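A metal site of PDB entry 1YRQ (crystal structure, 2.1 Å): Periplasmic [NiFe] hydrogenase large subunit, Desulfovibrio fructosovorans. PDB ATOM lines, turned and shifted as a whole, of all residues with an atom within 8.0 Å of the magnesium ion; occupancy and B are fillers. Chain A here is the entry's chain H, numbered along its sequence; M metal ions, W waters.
OG1 of Thr 355 lies within hydrogen-bond range of OE2 of Glu 53, at 2.7 Å.
O of Gly 547 sits close to ND1 of His 549 (3.4 Å).
O of Cys 546 lies within hydrogen-bond range of ND1 of His 549, 2.7 Å away.
The magnesium ion is bound by water W3 (2.0 Å), water W1 (2.0 Å), water W2 (2.0 Å), O of Leu 495 (2.1 Å), OE1 of Glu 53 (2.2 Å) and NE2 of His 549 (2.3 Å).
The magnesium ion has six donor atoms within binding distance.
Water W1 lies within hydrogen-bond range of the side-chain carboxylate of Glu 334 (2.6 Å), the side-chain amide oxygen of Gln 494 (2.7 Å) and the side-chain amino group of Lys 372 (3.1 Å).
Water W3 lies within hydrogen-bond range of OE2 of Glu 53 (2.5 Å) and NZ of Lys 372 (3.3 Å).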
ATOM      1  N   PHE A  49      14.459 -31.253   6.088  1.00  0.00           N
ATOM      2  CA  PHE A  49      12.989 -31.119   6.058  1.00  0.00           C
ATOM      3  C   PHE A  49      12.271 -32.269   5.342  1.00  0.00           C
ATOM      4  O   PHE A  49      12.637 -32.655   4.235  1.00  0.00           O
ATOM      5  CB  PHE A  49      12.580 -29.788   5.434  1.00  0.00           C
ATOM      6  CG  PHE A  49      11.085 -29.545   5.454  1.00  0.00           C
ATOM      7  CD1 PHE A  49      10.467 -29.011   6.573  1.00  0.00           C
ATOM      8  CD2 PHE A  49      10.314 -29.822   4.349  1.00  0.00           C
ATOM      9  CE1 PHE A  49       9.107 -28.766   6.597  1.00  0.00           C
ATOM     10  CE2 PHE A  49       8.951 -29.551   4.356  1.00  0.00           C
ATOM     11  CZ  PHE A  49       8.332 -29.039   5.476  1.00  0.00           C
ATOM     12  N   GLU A  53       3.458 -32.601   8.152  1.00  0.00           N
ATOM     13  CA  GLU A  53       2.243 -31.778   8.239  1.00  0.00           C
ATOM     14  C   GLU A  53       1.640 -31.462   6.871  1.00  0.00           C
ATOM     15  O   GLU A  53       0.422 -31.491   6.698  1.00  0.00           O
ATOM     16  CB  GLU A  53       2.542 -30.511   9.027  1.00  0.00           C
ATOM     17  CG  GLU A  53       3.071 -30.884  10.404  1.00  0.00           C
ATOM     18  CD  GLU A  53       3.807 -29.743  11.084  1.00  0.00           C
ATOM     19  OE1 GLU A  53       3.770 -29.716  12.329  1.00  0.00           O
ATOM     20  OE2 GLU A  53       4.411 -28.909  10.382  1.00  0.00           O
ATOM     21  N   GLU A 334       4.174 -20.928  17.835  1.00  0.00           N
ATOM     22  CA  GLU A 334       5.443 -21.163  17.163  1.00  0.00           C
ATOM     23  C   GLU A 334       5.809 -19.990  16.279  1.00  0.00           C
ATOM     24  O   GLU A 334       4.961 -19.447  15.541  1.00  0.00           O
ATOM     25  CB  GLU A 334       5.409 -22.455  16.321  1.00  0.00           C
ATOM     26  CG  GLU A 334       5.261 -23.741  17.129  1.00  0.00           C
ATOM     27  CD  GLU A 334       5.242 -24.979  16.238  1.00  0.00           C
ATOM     28  OE1 GLU A 334       4.264 -25.199  15.488  1.00  0.00           O
ATOM     29  OE2 GLU A 334       6.208 -25.756  16.262  1.00  0.00           O
ATOM     30  N   TYR A 341      11.159 -20.721   6.715  1.00  0.00           N
ATOM     31  CA  TYR A 341       9.759 -20.722   6.331  1.00  0.00           C
ATOM     32  C   TYR A 341       9.372 -19.387   5.729  1.00  0.00           C
ATOM     33  O   TYR A 341      10.097 -18.417   5.882  1.00  0.00           O
ATOM     34  CB  TYR A 341       8.832 -21.115   7.496  1.00  0.00           C
ATOM     35  CG  TYR A 341       9.077 -22.525   7.956  1.00  0.00           C
ATOM     36  CD1 TYR A 341       8.566 -23.617   7.235  1.00  0.00           C
ATOM     37  CD2 TYR A 341       9.855 -22.785   9.076  1.00  0.00           C
ATOM     38  CE1 TYR A 341       8.823 -24.925   7.653  1.00  0.00           C
ATOM     39  CE2 TYR A 341      10.116 -24.097   9.486  1.00  0.00           C
ATOM     40  CZ  TYR A 341       9.591 -25.149   8.772  1.00  0.00           C
ATOM     41  OH  TYR A 341       9.845 -26.420   9.219  1.00  0.00           O
ATOM     42  N   PRO A 350      -0.835 -23.593  17.393  1.00  0.00           N
ATOM     43  CA  PRO A 350      -0.805 -24.770  16.516  1.00  0.00           C
ATOM     44  C   PRO A 350      -2.133 -25.120  15.829  1.00  0.00           C
ATOM     45  O   PRO A 350      -2.118 -25.726  14.762  1.00  0.00           O
ATOM     46  CB  PRO A 350      -0.360 -25.925  17.447  1.00  0.00           C
ATOM     47  CG  PRO A 350       0.267 -25.273  18.625  1.00  0.00           C
ATOM     48  CD  PRO A 350      -0.363 -23.903  18.753  1.00  0.00           C
ATOM     49  N   GLY A 353      -1.702 -23.464  12.883  1.00  0.00           N
ATOM     50  CA  GLY A 353      -0.350 -23.646  12.399  1.00  0.00           C
ATOM     51  C   GLY A 353      -0.174 -23.602  10.892  1.00  0.00           C
ATOM     52  O   GLY A 353      -1.028 -24.048  10.136  1.00  0.00           O
ATOM     53  N   VAL A 354       0.981 -23.099  10.463  1.00  0.00           N
ATOM     54  CA  VAL A 354       1.284 -22.950   9.060  1.00  0.00           C
ATOM     55  C   VAL A 354       2.682 -23.547   8.780  1.00  0.00           C
ATOM     56  O   VAL A 354       3.646 -23.274   9.492  1.00  0.00           O
ATOM     57  CB  VAL A 354       1.249 -21.468   8.652  1.00  0.00           C
ATOM     58  CG1 VAL A 354       1.871 -21.281   7.288  1.00  0.00           C
ATOM     59  CG2 VAL A 354      -0.177 -20.968   8.657  1.00  0.00           C
ATOM     60  N   THR A 355       2.769 -24.373   7.740  1.00  0.00           N
ATOM     61  CA  THR A 355       4.046 -24.995   7.388  1.00  0.00           C
ATOM     62  C   THR A 355       4.382 -24.744   5.903  1.00  0.00           C
ATOM     63  O   THR A 355       4.004 -25.528   5.044  1.00  0.00           O
ATOM     64  CB  THR A 355       3.965 -26.484   7.715  1.00  0.00           C
ATOM     65  OG1 THR A 355       3.691 -26.602   9.128  1.00  0.00           O
ATOM     66  CG2 THR A 355       5.337 -27.168   7.525  1.00  0.00           C
ATOM     67  N   TRP A 370      15.463 -25.634  10.037  1.00  0.00           N
ATOM     68  CA  TRP A 370      14.205 -26.180   9.577  1.00  0.00           C
ATOM     69  C   TRP A 370      13.208 -26.402  10.707  1.00  0.00           C
ATOM     70  O   TRP A 370      12.074 -26.774  10.449  1.00  0.00           O
ATOM     71  CB  TRP A 370      14.393 -27.498   8.826  1.00  0.00           C
ATOM     72  CG  TRP A 370      14.909 -27.335   7.447  1.00  0.00           C
ATOM     73  CD1 TRP A 370      16.140 -27.719   6.996  1.00  0.00           C
ATOM     74  CD2 TRP A 370      14.203 -26.799   6.329  1.00  0.00           C
ATOM     75  NE1 TRP A 370      16.245 -27.436   5.653  1.00  0.00           N
ATOM     76  CE2 TRP A 370      15.074 -26.865   5.215  1.00  0.00           C
ATOM     77  CE3 TRP A 370      12.912 -26.263   6.141  1.00  0.00           C
ATOM     78  CZ2 TRP A 370      14.706 -26.418   3.941  1.00  0.00           C
ATOM     79  CZ3 TRP A 370      12.542 -25.825   4.871  1.00  0.00           C
ATOM     80  CH2 TRP A 370      13.438 -25.891   3.795  1.00  0.00           C
ATOM     81  N   MET A 371      13.623 -26.183  11.956  1.00  0.00           N
ATOM     82  CA  MET A 371      12.705 -26.264  13.069  1.00  0.00           C
ATOM     83  C   MET A 371      12.055 -24.906  13.257  1.00  0.00           C
ATOM     84  O   MET A 371      12.709 -23.893  13.071  1.00  0.00           O
ATOM     85  CB  MET A 371      13.428 -26.615  14.379  1.00  0.00           C
ATOM     86  CG  MET A 371      13.830 -28.054  14.492  1.00  0.00           C
ATOM     87  SD  MET A 371      14.255 -28.475  16.199  1.00  0.00           S
ATOM     88  CE  MET A 371      15.300 -29.860  15.924  1.00  0.00           C
ATOM     89  N   LYS A 372      10.776 -24.915  13.636  1.00  0.00           N
ATOM     90  CA  LYS A 372      10.093 -23.741  14.119  1.00  0.00           C
ATOM     91  C   LYS A 372      10.617 -23.407  15.507  1.00  0.00           C
ATOM     92  O   LYS A 372      11.363 -24.191  16.108  1.00  0.00           O
ATOM     93  CB  LYS A 372       8.568 -23.976  14.163  1.00  0.00           C
ATOM     94  CG  LYS A 372       7.905 -24.065  12.788  1.00  0.00           C
ATOM     95  CD  LYS A 372       6.407 -24.430  12.885  1.00  0.00           C
ATOM     96  CE  LYS A 372       5.824 -24.781  11.501  1.00  0.00           C
ATOM     97  NZ  LYS A 372       4.383 -25.093  11.596  1.00  0.00           N
ATOM     98  N   PRO A 374       9.069 -22.891  19.002  1.00  0.00           N
ATOM     99  CA  PRO A 374       7.916 -22.875  19.899  1.00  0.00           C
ATOM    100  C   PRO A 374       8.213 -22.023  21.134  1.00  0.00           C
ATOM    101  O   PRO A 374       9.311 -22.095  21.685  1.00  0.00           O
ATOM    102  CB  PRO A 374       7.702 -24.370  20.264  1.00  0.00           C
ATOM    103  CG  PRO A 374       8.728 -25.169  19.458  1.00  0.00           C
ATOM    104  CD  PRO A 374       9.796 -24.177  19.038  1.00  0.00           C
ATOM    105  N   SER A 480       2.981 -32.463  21.615  1.00  0.00           N
ATOM    106  CA  SER A 480       1.569 -32.293  21.301  1.00  0.00           C
ATOM    107  C   SER A 480       1.249 -32.364  19.811  1.00  0.00           C
ATOM    108  O   SER A 480       1.952 -31.774  18.974  1.00  0.00           O
ATOM    109  CB  SER A 480       0.989 -31.004  21.895  1.00  0.00           C
ATOM    110  OG  SER A 480       1.779 -29.901  21.535  1.00  0.00           O
ATOM    111  N   TRP A 482      -1.953 -31.589  17.039  1.00  0.00           N
ATOM    112  CA  TRP A 482      -3.114 -30.714  17.022  1.00  0.00           C
ATOM    113  C   TRP A 482      -3.862 -30.824  15.704  1.00  0.00           C
ATOM    114  O   TRP A 482      -3.288 -30.547  14.630  1.00  0.00           O
ATOM    115  CB  TRP A 482      -2.673 -29.268  17.195  1.00  0.00           C
ATOM    116  CG  TRP A 482      -1.768 -28.972  18.369  1.00  0.00           C
ATOM    117  CD1 TRP A 482      -0.433 -29.201  18.462  1.00  0.00           C
ATOM    118  CD2 TRP A 482      -2.139 -28.263  19.562  1.00  0.00           C
ATOM    119  NE1 TRP A 482       0.057 -28.720  19.659  1.00  0.00           N
ATOM    120  CE2 TRP A 482      -0.970 -28.141  20.353  1.00  0.00           C
ATOM    121  CE3 TRP A 482      -3.342 -27.744  20.050  1.00  0.00           C
ATOM    122  CZ2 TRP A 482      -0.975 -27.538  21.618  1.00  0.00           C
ATOM    123  CZ3 TRP A 482      -3.352 -27.123  21.302  1.00  0.00           C
ATOM    124  CH2 TRP A 482      -2.171 -27.037  22.070  1.00  0.00           C
ATOM    125  N   PHE A 493      -3.055 -30.331  10.478  1.00  0.00           N
ATOM    126  CA  PHE A 493      -2.471 -31.210  11.495  1.00  0.00           C
ATOM    127  C   PHE A 493      -1.078 -30.690  11.824  1.00  0.00           C
ATOM    128  O   PHE A 493      -0.247 -30.583  10.943  1.00  0.00           O
ATOM    129  CB  PHE A 493      -2.453 -32.673  11.047  1.00  0.00           C
ATOM    130  CG  PHE A 493      -2.326 -33.653  12.182  1.00  0.00           C
ATOM    131  CD1 PHE A 493      -1.119 -33.824  12.847  1.00  0.00           C
ATOM    132  CD2 PHE A 493      -3.420 -34.417  12.593  1.00  0.00           C
ATOM    133  CE1 PHE A 493      -1.000 -34.755  13.912  1.00  0.00           C
ATOM    134  CE2 PHE A 493      -3.302 -35.334  13.661  1.00  0.00           C
ATOM    135  CZ  PHE A 493      -2.111 -35.497  14.314  1.00  0.00           C
ATOM    136  N   GLN A 494      -0.841 -30.303  13.073  1.00  0.00           N
ATOM    137  CA  GLN A 494       0.437 -29.687  13.451  1.00  0.00           C
ATOM    138  C   GLN A 494       1.065 -30.458  14.605  1.00  0.00           C
ATOM    139  O   GLN A 494       0.356 -30.773  15.569  1.00  0.00           O
ATOM    140  CB  GLN A 494       0.211 -28.228  13.847  1.00  0.00           C
ATOM    141  CG  GLN A 494      -0.231 -27.327  12.686  1.00  0.00           C
ATOM    142  CD  GLN A 494       0.900 -27.022  11.689  1.00  0.00           C
ATOM    143  OE1 GLN A 494       2.008 -26.648  12.085  1.00  0.00           O
ATOM    144  NE2 GLN A 494       0.619 -27.190  10.403  1.00  0.00           N
ATOM    145  N   LEU A 495       2.344 -30.831  14.475  1.00  0.00           N
ATOM    146  CA  LEU A 495       3.113 -31.468  15.534  1.00  0.00           C
ATOM    147  C   LEU A 495       3.966 -30.379  16.139  1.00  0.00           C
ATOM    148  O   LEU A 495       4.512 -29.549  15.397  1.00  0.00           O
ATOM    149  CB  LEU A 495       4.024 -32.571  14.961  1.00  0.00           C
ATOM    150  CG  LEU A 495       3.433 -33.853  14.324  1.00  0.00           C
ATOM    151  CD1 LEU A 495       2.769 -33.588  13.006  1.00  0.00           C
ATOM    152  CD2 LEU A 495       4.561 -34.877  14.095  1.00  0.00           C
ATOM    153  N   VAL A 496       4.028 -30.313  17.475  1.00  0.00           N
ATOM    154  CA  VAL A 496       4.968 -29.423  18.166  1.00  0.00           C
ATOM    155  C   VAL A 496       5.674 -30.350  19.122  1.00  0.00           C
ATOM    156  O   VAL A 496       5.038 -30.859  20.048  1.00  0.00           O
ATOM    157  CB  VAL A 496       4.275 -28.326  18.993  1.00  0.00           C
ATOM    158  CG1 VAL A 496       5.336 -27.416  19.670  1.00  0.00           C
ATOM    159  CG2 VAL A 496       3.283 -27.477  18.152  1.00  0.00           C
ATOM    160  N   VAL A 497       6.959 -30.599  18.897  1.00  0.00           N
ATOM    161  CA  VAL A 497       7.663 -31.804  19.369  1.00  0.00           C
ATOM    162  C   VAL A 497       8.764 -31.437  20.386  1.00  0.00           C
ATOM    163  O   VAL A 497       9.343 -30.368  20.281  1.00  0.00           O
ATOM    164  CB  VAL A 497       8.220 -32.633  18.164  1.00  0.00           C
ATOM    165  CG1 VAL A 497       8.814 -34.015  18.582  1.00  0.00           C
ATOM    166  CG2 VAL A 497       7.070 -32.869  17.159  1.00  0.00           C
ATOM    167  N   THR A 500      11.650 -29.752  19.309  1.00  0.00           N
ATOM    168  CA  THR A 500      11.368 -28.455  18.656  1.00  0.00           C
ATOM    169  C   THR A 500      11.498 -27.391  19.718  1.00  0.00           C
ATOM    170  O   THR A 500      12.008 -26.295  19.486  1.00  0.00           O
ATOM    171  CB  THR A 500       9.946 -28.359  18.077  1.00  0.00           C
ATOM    172  OG1 THR A 500       9.620 -29.536  17.323  1.00  0.00           O
ATOM    173  CG2 THR A 500       9.906 -27.210  17.039  1.00  0.00           C
ATOM    174  N   CYS A 546      12.228 -35.737  14.798  1.00  0.00           N
ATOM    175  CA  CYS A 546      11.129 -35.320  15.690  1.00  0.00           C
ATOM    176  C   CYS A 546      10.966 -33.787  15.618  1.00  0.00           C
ATOM    177  O   CYS A 546       9.847 -33.277  15.444  1.00  0.00           O
ATOM    178  CB  CYS A 546      11.396 -35.740  17.137  1.00  0.00           C
ATOM    179  SG  CYS A 546      10.615 -37.289  17.637  1.00  0.00           S
ATOM    180  N   GLY A 547      12.073 -33.063  15.744  1.00  0.00           N
ATOM    181  CA  GLY A 547      12.076 -31.600  15.784  1.00  0.00           C
ATOM    182  C   GLY A 547      11.432 -30.931  14.594  1.00  0.00           C
ATOM    183  O   GLY A 547      10.640 -30.000  14.758  1.00  0.00           O
ATOM    184  N   VAL A 548      11.751 -31.402  13.399  1.00  0.00           N
ATOM    185  CA  VAL A 548      11.348 -30.740  12.158  1.00  0.00           C
ATOM    186  C   VAL A 548      10.128 -31.427  11.534  1.00  0.00           C
ATOM    187  O   VAL A 548       9.235 -30.755  10.975  1.00  0.00           O
ATOM    188  CB  VAL A 548      12.489 -30.811  11.108  1.00  0.00           C
ATOM    189  CG1 VAL A 548      12.035 -30.197   9.832  1.00  0.00           C
ATOM    190  CG2 VAL A 548      13.751 -30.113  11.608  1.00  0.00           C
ATOM    191  N   HIS A 549      10.105 -32.758  11.646  1.00  0.00           N
ATOM    192  CA  HIS A 549       9.074 -33.561  11.022  1.00  0.00           C
ATOM    193  C   HIS A 549       8.703 -32.999   9.628  1.00  0.00           C
ATOM    194  O   HIS A 549       7.539 -32.830   9.227  1.00  0.00           O
ATOM    195  CB  HIS A 549       7.840 -33.695  11.942  1.00  0.00           C
ATOM    196  CG  HIS A 549       7.471 -32.419  12.625  1.00  0.00           C
ATOM    197  ND1 HIS A 549       8.030 -32.025  13.819  1.00  0.00           N
ATOM    198  CD2 HIS A 549       6.610 -31.433  12.253  1.00  0.00           C
ATOM    199  CE1 HIS A 549       7.529 -30.856  14.169  1.00  0.00           C
ATOM    200  NE2 HIS A 549       6.668 -30.467  13.235  1.00  0.00           N
ATOM    201  OXT HIS A 549       9.560 -32.686   8.791  1.00  0.00           O
HETATM  202 MG    MG M   1       5.313 -28.703  13.598  1.00  0.00          MG
HETATM  203  O   HOH W   1       4.003 -27.173  13.868  1.00  0.00           O
HETATM  204  O   HOH W   2       6.733 -27.716  14.692  1.00  0.00           O
HETATM  205  O   HOH W   3       6.074 -27.891  11.899  1.00  0.00           O
